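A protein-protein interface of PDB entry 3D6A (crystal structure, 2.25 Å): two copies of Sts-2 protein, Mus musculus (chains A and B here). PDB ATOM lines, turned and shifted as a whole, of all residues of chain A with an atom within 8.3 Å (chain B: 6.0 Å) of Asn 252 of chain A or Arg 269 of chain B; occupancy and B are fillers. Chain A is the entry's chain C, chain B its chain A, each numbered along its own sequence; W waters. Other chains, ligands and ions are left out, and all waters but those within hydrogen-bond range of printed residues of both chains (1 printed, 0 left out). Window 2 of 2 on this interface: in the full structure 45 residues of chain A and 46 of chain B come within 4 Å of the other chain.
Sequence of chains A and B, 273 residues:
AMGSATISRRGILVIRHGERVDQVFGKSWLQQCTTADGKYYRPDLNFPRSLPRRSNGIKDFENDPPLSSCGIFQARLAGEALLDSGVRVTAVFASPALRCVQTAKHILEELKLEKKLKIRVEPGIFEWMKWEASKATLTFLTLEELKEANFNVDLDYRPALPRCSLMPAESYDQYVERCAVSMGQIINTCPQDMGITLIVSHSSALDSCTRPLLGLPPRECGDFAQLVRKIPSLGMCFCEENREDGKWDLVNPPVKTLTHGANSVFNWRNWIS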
ATOM      1  N   LEU A  13      25.790  18.806  13.651  1.00  0.00           N
ATOM      2  CA  LEU A  13      24.698  19.389  12.872  1.00  0.00           C
ATOM      3  C   LEU A  13      23.860  18.284  12.240  1.00  0.00           C
ATOM      4  O   LEU A  13      24.336  17.601  11.327  1.00  0.00           O
ATOM      5  CB  LEU A  13      25.269  20.310  11.784  1.00  0.00           C
ATOM      6  CG  LEU A  13      24.338  21.198  10.937  1.00  0.00           C
ATOM      7  CD1 LEU A  13      23.452  22.080  11.811  1.00  0.00           C
ATOM      8  CD2 LEU A  13      25.125  22.054   9.961  1.00  0.00           C
ATOM      9  N   ILE A 196      32.951  20.747  12.980  1.00  0.00           N
ATOM     10  CA  ILE A 196      31.556  20.336  12.976  1.00  0.00           C
ATOM     11  C   ILE A 196      31.357  18.999  12.259  1.00  0.00           C
ATOM     12  O   ILE A 196      31.837  18.806  11.146  1.00  0.00           O
ATOM     13  CB  ILE A 196      30.681  21.461  12.393  1.00  0.00           C
ATOM     14  CG1 ILE A 196      30.631  22.627  13.389  1.00  0.00           C
ATOM     15  CG2 ILE A 196      29.279  20.962  12.063  1.00  0.00           C
ATOM     16  CD1 ILE A 196      30.209  23.946  12.803  1.00  0.00           C
ATOM     17  N   LEU A 206      16.263  14.652  14.047  1.00  0.00           N
ATOM     18  CA  LEU A 206      16.514  15.965  14.670  1.00  0.00           C
ATOM     19  C   LEU A 206      16.133  15.964  16.147  1.00  0.00           C
ATOM     20  O   LEU A 206      16.598  16.805  16.921  1.00  0.00           O
ATOM     21  CB  LEU A 206      15.788  17.102  13.933  1.00  0.00           C
ATOM     22  CG  LEU A 206      16.460  17.729  12.702  1.00  0.00           C
ATOM     23  CD1 LEU A 206      16.457  16.798  11.462  1.00  0.00           C
ATOM     24  CD2 LEU A 206      15.812  19.068  12.384  1.00  0.00           C
ATOM     25  N   ARG A 219      10.757  11.754  24.329  1.00  0.00           N
ATOM     26  CA  ARG A 219       9.443  12.387  24.397  1.00  0.00           C
ATOM     27  C   ARG A 219       8.331  11.340  24.374  1.00  0.00           C
ATOM     28  O   ARG A 219       8.540  10.225  23.904  1.00  0.00           O
ATOM     29  CB  ARG A 219       9.255  13.338  23.211  1.00  0.00           C
ATOM     30  CG  ARG A 219      10.282  14.446  23.104  1.00  0.00           C
ATOM     31  CD  ARG A 219       9.883  15.447  22.025  1.00  0.00           C
ATOM     32  NE  ARG A 219      10.952  16.397  21.725  1.00  0.00           N
ATOM     33  CZ  ARG A 219      11.053  17.625  22.238  1.00  0.00           C
ATOM     34  NH1 ARG A 219      10.140  18.086  23.091  1.00  0.00           N
ATOM     35  NH2 ARG A 219      12.072  18.403  21.886  1.00  0.00           N
ATOM     36  N   MET A 236      17.485  21.747  10.040  1.00  0.00           N
ATOM     37  CA  MET A 236      18.689  21.507  10.827  1.00  0.00           C
ATOM     38  C   MET A 236      18.471  21.685  12.325  1.00  0.00           C
ATOM     39  O   MET A 236      17.619  22.469  12.773  1.00  0.00           O
ATOM     40  CB  MET A 236      19.840  22.422  10.390  1.00  0.00           C
ATOM     41  CG  MET A 236      20.288  22.190   8.993  1.00  0.00           C
ATOM     42  SD  MET A 236      21.515  23.379   8.472  1.00  0.00           S
ATOM     43  CE  MET A 236      21.639  22.884   6.735  1.00  0.00           C
ATOM     44  N   CYS A 237      19.274  20.932  13.068  1.00  0.00           N
ATOM     45  CA  CYS A 237      19.317  20.961  14.508  1.00  0.00           C
ATOM     46  C   CYS A 237      20.805  20.945  14.868  1.00  0.00           C
ATOM     47  O   CYS A 237      21.561  20.126  14.344  1.00  0.00           O
ATOM     48  CB  CYS A 237      18.620  19.718  15.055  1.00  0.00           C
ATOM     49  SG  CYS A 237      18.493  19.712  16.809  1.00  0.00           S
ATOM     50  N   PHE A 238      21.225  21.862  15.735  1.00  0.00           N
ATOM     51  CA  PHE A 238      22.645  22.026  16.030  1.00  0.00           C
ATOM     52  C   PHE A 238      22.945  21.959  17.540  1.00  0.00           C
ATOM     53  O   PHE A 238      22.367  22.704  18.335  1.00  0.00           O
ATOM     54  CB  PHE A 238      23.144  23.332  15.410  1.00  0.00           C
ATOM     55  CG  PHE A 238      24.632  23.538  15.509  1.00  0.00           C
ATOM     56  CD1 PHE A 238      25.528  22.556  15.083  1.00  0.00           C
ATOM     57  CD2 PHE A 238      25.142  24.742  15.984  1.00  0.00           C
ATOM     58  CE1 PHE A 238      26.897  22.758  15.158  1.00  0.00           C
ATOM     59  CE2 PHE A 238      26.503  24.947  16.063  1.00  0.00           C
ATOM     60  CZ  PHE A 238      27.388  23.943  15.642  1.00  0.00           C
ATOM     61  N   CYS A 239      23.836  21.042  17.906  1.00  0.00           N
ATOM     62  CA  CYS A 239      24.271  20.852  19.288  1.00  0.00           C
ATOM     63  C   CYS A 239      25.771  21.076  19.405  1.00  0.00           C
ATOM     64  O   CYS A 239      26.548  20.457  18.676  1.00  0.00           O
ATOM     65  CB  CYS A 239      23.933  19.441  19.774  1.00  0.00           C
ATOM     66  SG  CYS A 239      22.161  19.140  19.888  1.00  0.00           S
ATOM     67  N   GLU A 240      26.157  21.967  20.318  1.00  0.00           N
ATOM     68  CA  GLU A 240      27.561  22.217  20.655  1.00  0.00           C
ATOM     69  C   GLU A 240      27.965  21.544  21.967  1.00  0.00           C
ATOM     70  O   GLU A 240      27.154  21.406  22.881  1.00  0.00           O
ATOM     71  CB  GLU A 240      27.829  23.715  20.772  1.00  0.00           C
ATOM     72  CG  GLU A 240      27.996  24.421  19.447  1.00  0.00           C
ATOM     73  CD  GLU A 240      28.696  25.759  19.582  1.00  0.00           C
ATOM     74  OE1 GLU A 240      28.387  26.527  20.529  1.00  0.00           O
ATOM     75  OE2 GLU A 240      29.559  26.038  18.722  1.00  0.00           O
ATOM     76  N   ASP A 249      24.926  21.386  24.489  1.00  0.00           N
ATOM     77  CA  ASP A 249      23.939  22.465  24.402  1.00  0.00           C
ATOM     78  C   ASP A 249      23.329  22.547  23.006  1.00  0.00           C
ATOM     79  O   ASP A 249      24.055  22.602  22.015  1.00  0.00           O
ATOM     80  CB  ASP A 249      24.599  23.820  24.713  1.00  0.00           C
ATOM     81  CG  ASP A 249      25.107  23.916  26.141  1.00  0.00           C
ATOM     82  OD1 ASP A 249      24.290  24.258  27.029  1.00  0.00           O
ATOM     83  OD2 ASP A 249      26.321  23.672  26.364  1.00  0.00           O
ATOM     84  N   LEU A 250      21.998  22.569  22.944  1.00  0.00           N
ATOM     85  CA  LEU A 250      21.275  22.854  21.707  1.00  0.00           C
ATOM     86  C   LEU A 250      21.402  24.336  21.411  1.00  0.00           C
ATOM     87  O   LEU A 250      21.068  25.166  22.250  1.00  0.00           O
ATOM     88  CB  LEU A 250      19.795  22.486  21.849  1.00  0.00           C
ATOM     89  CG  LEU A 250      18.996  22.238  20.566  1.00  0.00           C
ATOM     90  CD1 LEU A 250      19.358  20.907  19.972  1.00  0.00           C
ATOM     91  CD2 LEU A 250      17.516  22.253  20.848  1.00  0.00           C
ATOM     92  N   VAL A 251      21.872  24.656  20.212  1.00  0.00           N
ATOM     93  CA  VAL A 251      22.277  26.018  19.831  1.00  0.00           C
ATOM     94  C   VAL A 251      21.719  26.393  18.438  1.00  0.00           C
ATOM     95  O   VAL A 251      21.222  25.531  17.711  1.00  0.00           O
ATOM     96  CB  VAL A 251      23.842  26.129  19.904  1.00  0.00           C
ATOM     97  CG1 VAL A 251      24.414  27.212  18.994  1.00  0.00           C
ATOM     98  CG2 VAL A 251      24.299  26.340  21.353  1.00  0.00           C
ATOM     99  N   ASN A 252      21.774  27.680  18.099  1.00  0.00           N
ATOM    100  CA  ASN A 252      21.464  28.175  16.755  1.00  0.00           C
ATOM    101  C   ASN A 252      22.384  27.582  15.687  1.00  0.00           C
ATOM    102  O   ASN A 252      23.602  27.684  15.815  1.00  0.00           O
ATOM    103  CB  ASN A 252      21.614  29.697  16.716  1.00  0.00           C
ATOM    104  CG  ASN A 252      20.862  30.384  17.831  1.00  0.00           C
ATOM    105  OD1 ASN A 252      19.650  30.599  17.731  1.00  0.00           O
ATOM    106  ND2 ASN A 252      21.575  30.737  18.907  1.00  0.00           N
ATOM    107  N   PRO A 253      21.810  26.967  14.631  1.00  0.00           N
ATOM    108  CA  PRO A 253      22.619  26.429  13.512  1.00  0.00           C
ATOM    109  C   PRO A 253      23.484  27.501  12.826  1.00  0.00           C
ATOM    110  O   PRO A 253      23.109  28.673  12.817  1.00  0.00           O
ATOM    111  CB  PRO A 253      21.568  25.903  12.524  1.00  0.00           C
ATOM    112  CG  PRO A 253      20.311  25.746  13.307  1.00  0.00           C
ATOM    113  CD  PRO A 253      20.363  26.735  14.442  1.00  0.00           C
ATOM    114  N   PRO A 254      24.632  27.104  12.245  1.00  0.00           N
ATOM    115  CA  PRO A 254      25.533  28.093  11.640  1.00  0.00           C
ATOM    116  C   PRO A 254      25.025  28.705  10.316  1.00  0.00           C
ATOM    117  O   PRO A 254      25.634  29.654   9.794  1.00  0.00           O
ATOM    118  CB  PRO A 254      26.811  27.284  11.401  1.00  0.00           C
ATOM    119  CG  PRO A 254      26.334  25.896  11.208  1.00  0.00           C
ATOM    120  CD  PRO A 254      25.172  25.736  12.131  1.00  0.00           C
ATOM    121  N   VAL A 255      23.935  28.160   9.774  1.00  0.00           N
ATOM    122  CA  VAL A 255      23.336  28.707   8.564  1.00  0.00           C
ATOM    123  C   VAL A 255      21.863  29.047   8.769  1.00  0.00           C
ATOM    124  O   VAL A 255      21.187  28.481   9.633  1.00  0.00           O
ATOM    125  CB  VAL A 255      23.533  27.782   7.327  1.00  0.00           C
ATOM    126  CG1 VAL A 255      25.001  27.622   7.023  1.00  0.00           C
ATOM    127  CG2 VAL A 255      22.875  26.432   7.530  1.00  0.00           C
ATOM    128  N   LYS A 256      21.381  29.998   7.983  1.00  0.00           N
ATOM    129  CA  LYS A 256      19.984  30.373   8.019  1.00  0.00           C
ATOM    130  C   LYS A 256      19.060  29.270   7.490  1.00  0.00           C
ATOM    131  O   LYS A 256      19.484  28.287   6.853  1.00  0.00           O
ATOM    132  CB  LYS A 256      19.755  31.671   7.227  1.00  0.00           C
ATOM    133  CG  LYS A 256      20.511  32.903   7.754  1.00  0.00           C
ATOM    134  CD  LYS A 256      20.326  33.098   9.259  1.00  0.00           C
ATOM    135  CE  LYS A 256      20.616  34.532   9.695  1.00  0.00           C
ATOM    136  NZ  LYS A 256      21.960  35.015   9.223  1.00  0.00           N
ATOM    137  N   ASN B 267      12.498  26.922  12.619  1.00  0.00           N
ATOM    138  CA  ASN B 267      13.521  27.044  13.641  1.00  0.00           C
ATOM    139  C   ASN B 267      13.231  26.043  14.747  1.00  0.00           C
ATOM    140  O   ASN B 267      12.211  26.143  15.434  1.00  0.00           O
ATOM    141  CB  ASN B 267      13.613  28.478  14.176  1.00  0.00           C
ATOM    142  CG  ASN B 267      14.832  28.692  15.049  1.00  0.00           C
ATOM    143  OD1 ASN B 267      15.872  29.167  14.578  1.00  0.00           O
ATOM    144  ND2 ASN B 267      14.727  28.318  16.323  1.00  0.00           N
ATOM    145  N   TRP B 268      14.131  25.070  14.889  1.00  0.00           N
ATOM    146  CA  TRP B 268      13.941  23.940  15.795  1.00  0.00           C
ATOM    147  C   TRP B 268      13.830  24.357  17.266  1.00  0.00           C
ATOM    148  O   TRP B 268      12.996  23.826  18.003  1.00  0.00           O
ATOM    149  CB  TRP B 268      15.062  22.915  15.615  1.00  0.00           C
ATOM    150  CG  TRP B 268      14.905  21.678  16.465  1.00  0.00           C
ATOM    151  CD1 TRP B 268      15.764  21.237  17.435  1.00  0.00           C
ATOM    152  CD2 TRP B 268      13.819  20.730  16.428  1.00  0.00           C
ATOM    153  NE1 TRP B 268      15.292  20.069  17.993  1.00  0.00           N
ATOM    154  CE2 TRP B 268      14.101  19.738  17.399  1.00  0.00           C
ATOM    155  CE3 TRP B 268      12.640  20.624  15.667  1.00  0.00           C
ATOM    156  CZ2 TRP B 268      13.248  18.652  17.633  1.00  0.00           C
ATOM    157  CZ3 TRP B 268      11.789  19.544  15.902  1.00  0.00           C
ATOM    158  CH2 TRP B 268      12.101  18.572  16.882  1.00  0.00           C
ATOM    159  N   ARG B 269      14.675  25.298  17.677  1.00  0.00           N
ATOM    160  CA  ARG B 269      14.673  25.811  19.047  1.00  0.00           C
ATOM    161  C   ARG B 269      13.375  26.543  19.389  1.00  0.00           C
ATOM    162  O   ARG B 269      12.827  26.367  20.480  1.00  0.00           O
ATOM    163  CB  ARG B 269      15.897  26.695  19.291  1.00  0.00           C
ATOM    164  CG  ARG B 269      17.196  25.916  19.442  1.00  0.00           C
ATOM    165  CD  ARG B 269      18.341  26.843  19.789  1.00  0.00           C
ATOM    166  NE  ARG B 269      17.988  27.770  20.864  1.00  0.00           N
ATOM    167  CZ  ARG B 269      18.794  28.716  21.341  1.00  0.00           C
ATOM    168  NH1 ARG B 269      20.017  28.870  20.844  1.00  0.00           N
ATOM    169  NH2 ARG B 269      18.379  29.515  22.317  1.00  0.00           N
ATOM    170  N   ASN B 270      12.889  27.347  18.446  1.00  0.00           N
ATOM    171  CA  ASN B 270      11.547  27.927  18.507  1.00  0.00           C
ATOM    172  C   ASN B 270      10.474  26.840  18.666  1.00  0.00           C
ATOM    173  O   ASN B 270       9.773  26.793  19.679  1.00  0.00           O
ATOM    174  CB  ASN B 270      11.254  28.755  17.240  1.00  0.00           C
ATOM    175  CG  ASN B 270      12.048  30.060  17.168  1.00  0.00           C
ATOM    176  OD1 ASN B 270      13.025  30.274  17.901  1.00  0.00           O
ATOM    177  ND2 ASN B 270      11.626  30.941  16.262  1.00  0.00           N
ATOM    178  N   TRP B 271      10.374  25.973  17.657  1.00  0.00           N
ATOM    179  CA  TRP B 271       9.414  24.861  17.596  1.00  0.00           C
ATOM    180  C   TRP B 271       9.157  24.152  18.923  1.00  0.00           C
ATOM    181  O   TRP B 271       8.002  23.913  19.285  1.00  0.00           O
ATOM    182  CB  TRP B 271       9.903  23.816  16.587  1.00  0.00           C
ATOM    183  CG  TRP B 271       9.116  23.697  15.309  1.00  0.00           C
ATOM    184  CD1 TRP B 271       8.436  22.592  14.872  1.00  0.00           C
ATOM    185  CD2 TRP B 271       8.956  24.698  14.284  1.00  0.00           C
ATOM    186  NE1 TRP B 271       7.860  22.842  13.647  1.00  0.00           N
ATOM    187  CE2 TRP B 271       8.159  24.124  13.263  1.00  0.00           C
ATOM    188  CE3 TRP B 271       9.402  26.023  14.133  1.00  0.00           C
ATOM    189  CZ2 TRP B 271       7.795  24.832  12.105  1.00  0.00           C
ATOM    190  CZ3 TRP B 271       9.041  26.725  12.986  1.00  0.00           C
ATOM    191  CH2 TRP B 271       8.241  26.126  11.986  1.00  0.00           C
ATOM    192  N   ILE B 272      10.236  23.820  19.633  1.00  0.00           N
ATOM    193  CA  ILE B 272      10.167  22.938  20.802  1.00  0.00           C
ATOM    194  C   ILE B 272       9.857  23.620  22.145  1.00  0.00           C
ATOM    195  O   ILE B 272       9.663  22.933  23.156  1.00  0.00           O
ATOM    196  CB  ILE B 272      11.457  22.075  20.946  1.00  0.00           C
ATOM    197  CG1 ILE B 272      12.703  22.965  21.060  1.00  0.00           C
ATOM    198  CG2 ILE B 272      11.569  21.095  19.787  1.00  0.00           C
ATOM    199  CD1 ILE B 272      13.843  22.340  21.831  1.00  0.00           C
ATOM    200  N   SER B 273       9.798  24.954  22.155  1.00  0.00           N
ATOM    201  CA  SER B 273       9.559  25.711  23.391  1.00  0.00           C
ATOM    202  C   SER B 273       8.137  25.530  23.936  1.00  0.00           C
ATOM    203  O   SER B 273       7.152  25.653  23.202  1.00  0.00           O
ATOM    204  CB  SER B 273       9.869  27.195  23.185  1.00  0.00           C
ATOM    205  OG  SER B 273       8.986  27.775  22.235  1.00  0.00           O
HETATM  206  O   HOH W   1      17.725  28.452  16.695  1.00  0.00           O
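NE1 of Trp 268 of chain B lies close to SG of Cys 237 of chain A (3.4 Å).
NH1 of Arg 269 of chain B sits close to ND2 of Asn 252 of chain A (3.1 Å).
The side-chain amide nitrogen (ND2) of Asn 267 of chain B lies close to the backbone NH (N) of Arg 269 of chain B, 3.3 Å away.
The side-chain sulfur (SG) of Cys 237 of chain A sits at hydrogen-bond distance from the backbone carbonyl oxygen (O) of Leu 206 of chain A, 3.5 Å away.
N of Val 251 of chain A is in hydrogen-bond range of O of Phe 238 of chain A, 2.8 Å away.
Among the printed residues, merely in contact across the chains: Arg 219 of chain A with Ile 272 of chain B (3.5 Å), Val 251 of chain A with Arg 269 of chain B (3.7 Å), Leu 206 of chain A with Trp 268 of chain B (3.7 Å), Leu 250 of chain A with Ile 272 of chain B (3.8 Å), Met 236 of chain A with Trp 268 of chain B (3.8 Å), Leu 250 of chain A with Arg 269 of chain B (3.9 Å) and Leu 250 of chain A with Trp 268 of chain B (3.97 Å).
Of chain B, only Arg 269 (3.1 Å) comes within 4 Å of Asn 252 of chain A.
Of chain A, only Leu 250, Val 251 and Asn 252 come within 4 Å of Arg 269 of chain B.
Of the printed residues of chain A, Ile 272 of chain B touches Arg 219 and Leu 250.
Of the printed residues of chain B, Leu 206 of chain A touches Trp 268.
The nearest residue of chain A that does not touch Arg 269 of chain B is Pro 253 of chain A (5.7 Å).
Hydrophobic or aromatic side chains of chain B within 4 Å of the printed part of chain A: Trp 268 and Ile 272.
Of the 17 printed residues of chain A, 7 touch a printed residue of chain B.
Printed residues of chain A that touch a printed residue of chain B: Leu 206, Arg 219, Met 236, Cys 237, Leu 250, Val 251 and Asn 252.
Among the printed residues, no Asp or Glu carboxylate lies within 4 Å of a Lys or Arg side-chain nitrogen of the other chain.
No position is printed for both chains.
Of the 9 pairs that touch across the chains among the printed residues, none has its exchanged pair printed and touching as well.
Water W1 lies within hydrogen-bond range of OD1 of Asn 267 of chain B (2.9 Å) and OD1 of Asn 252 of chain A (3.1 Å).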
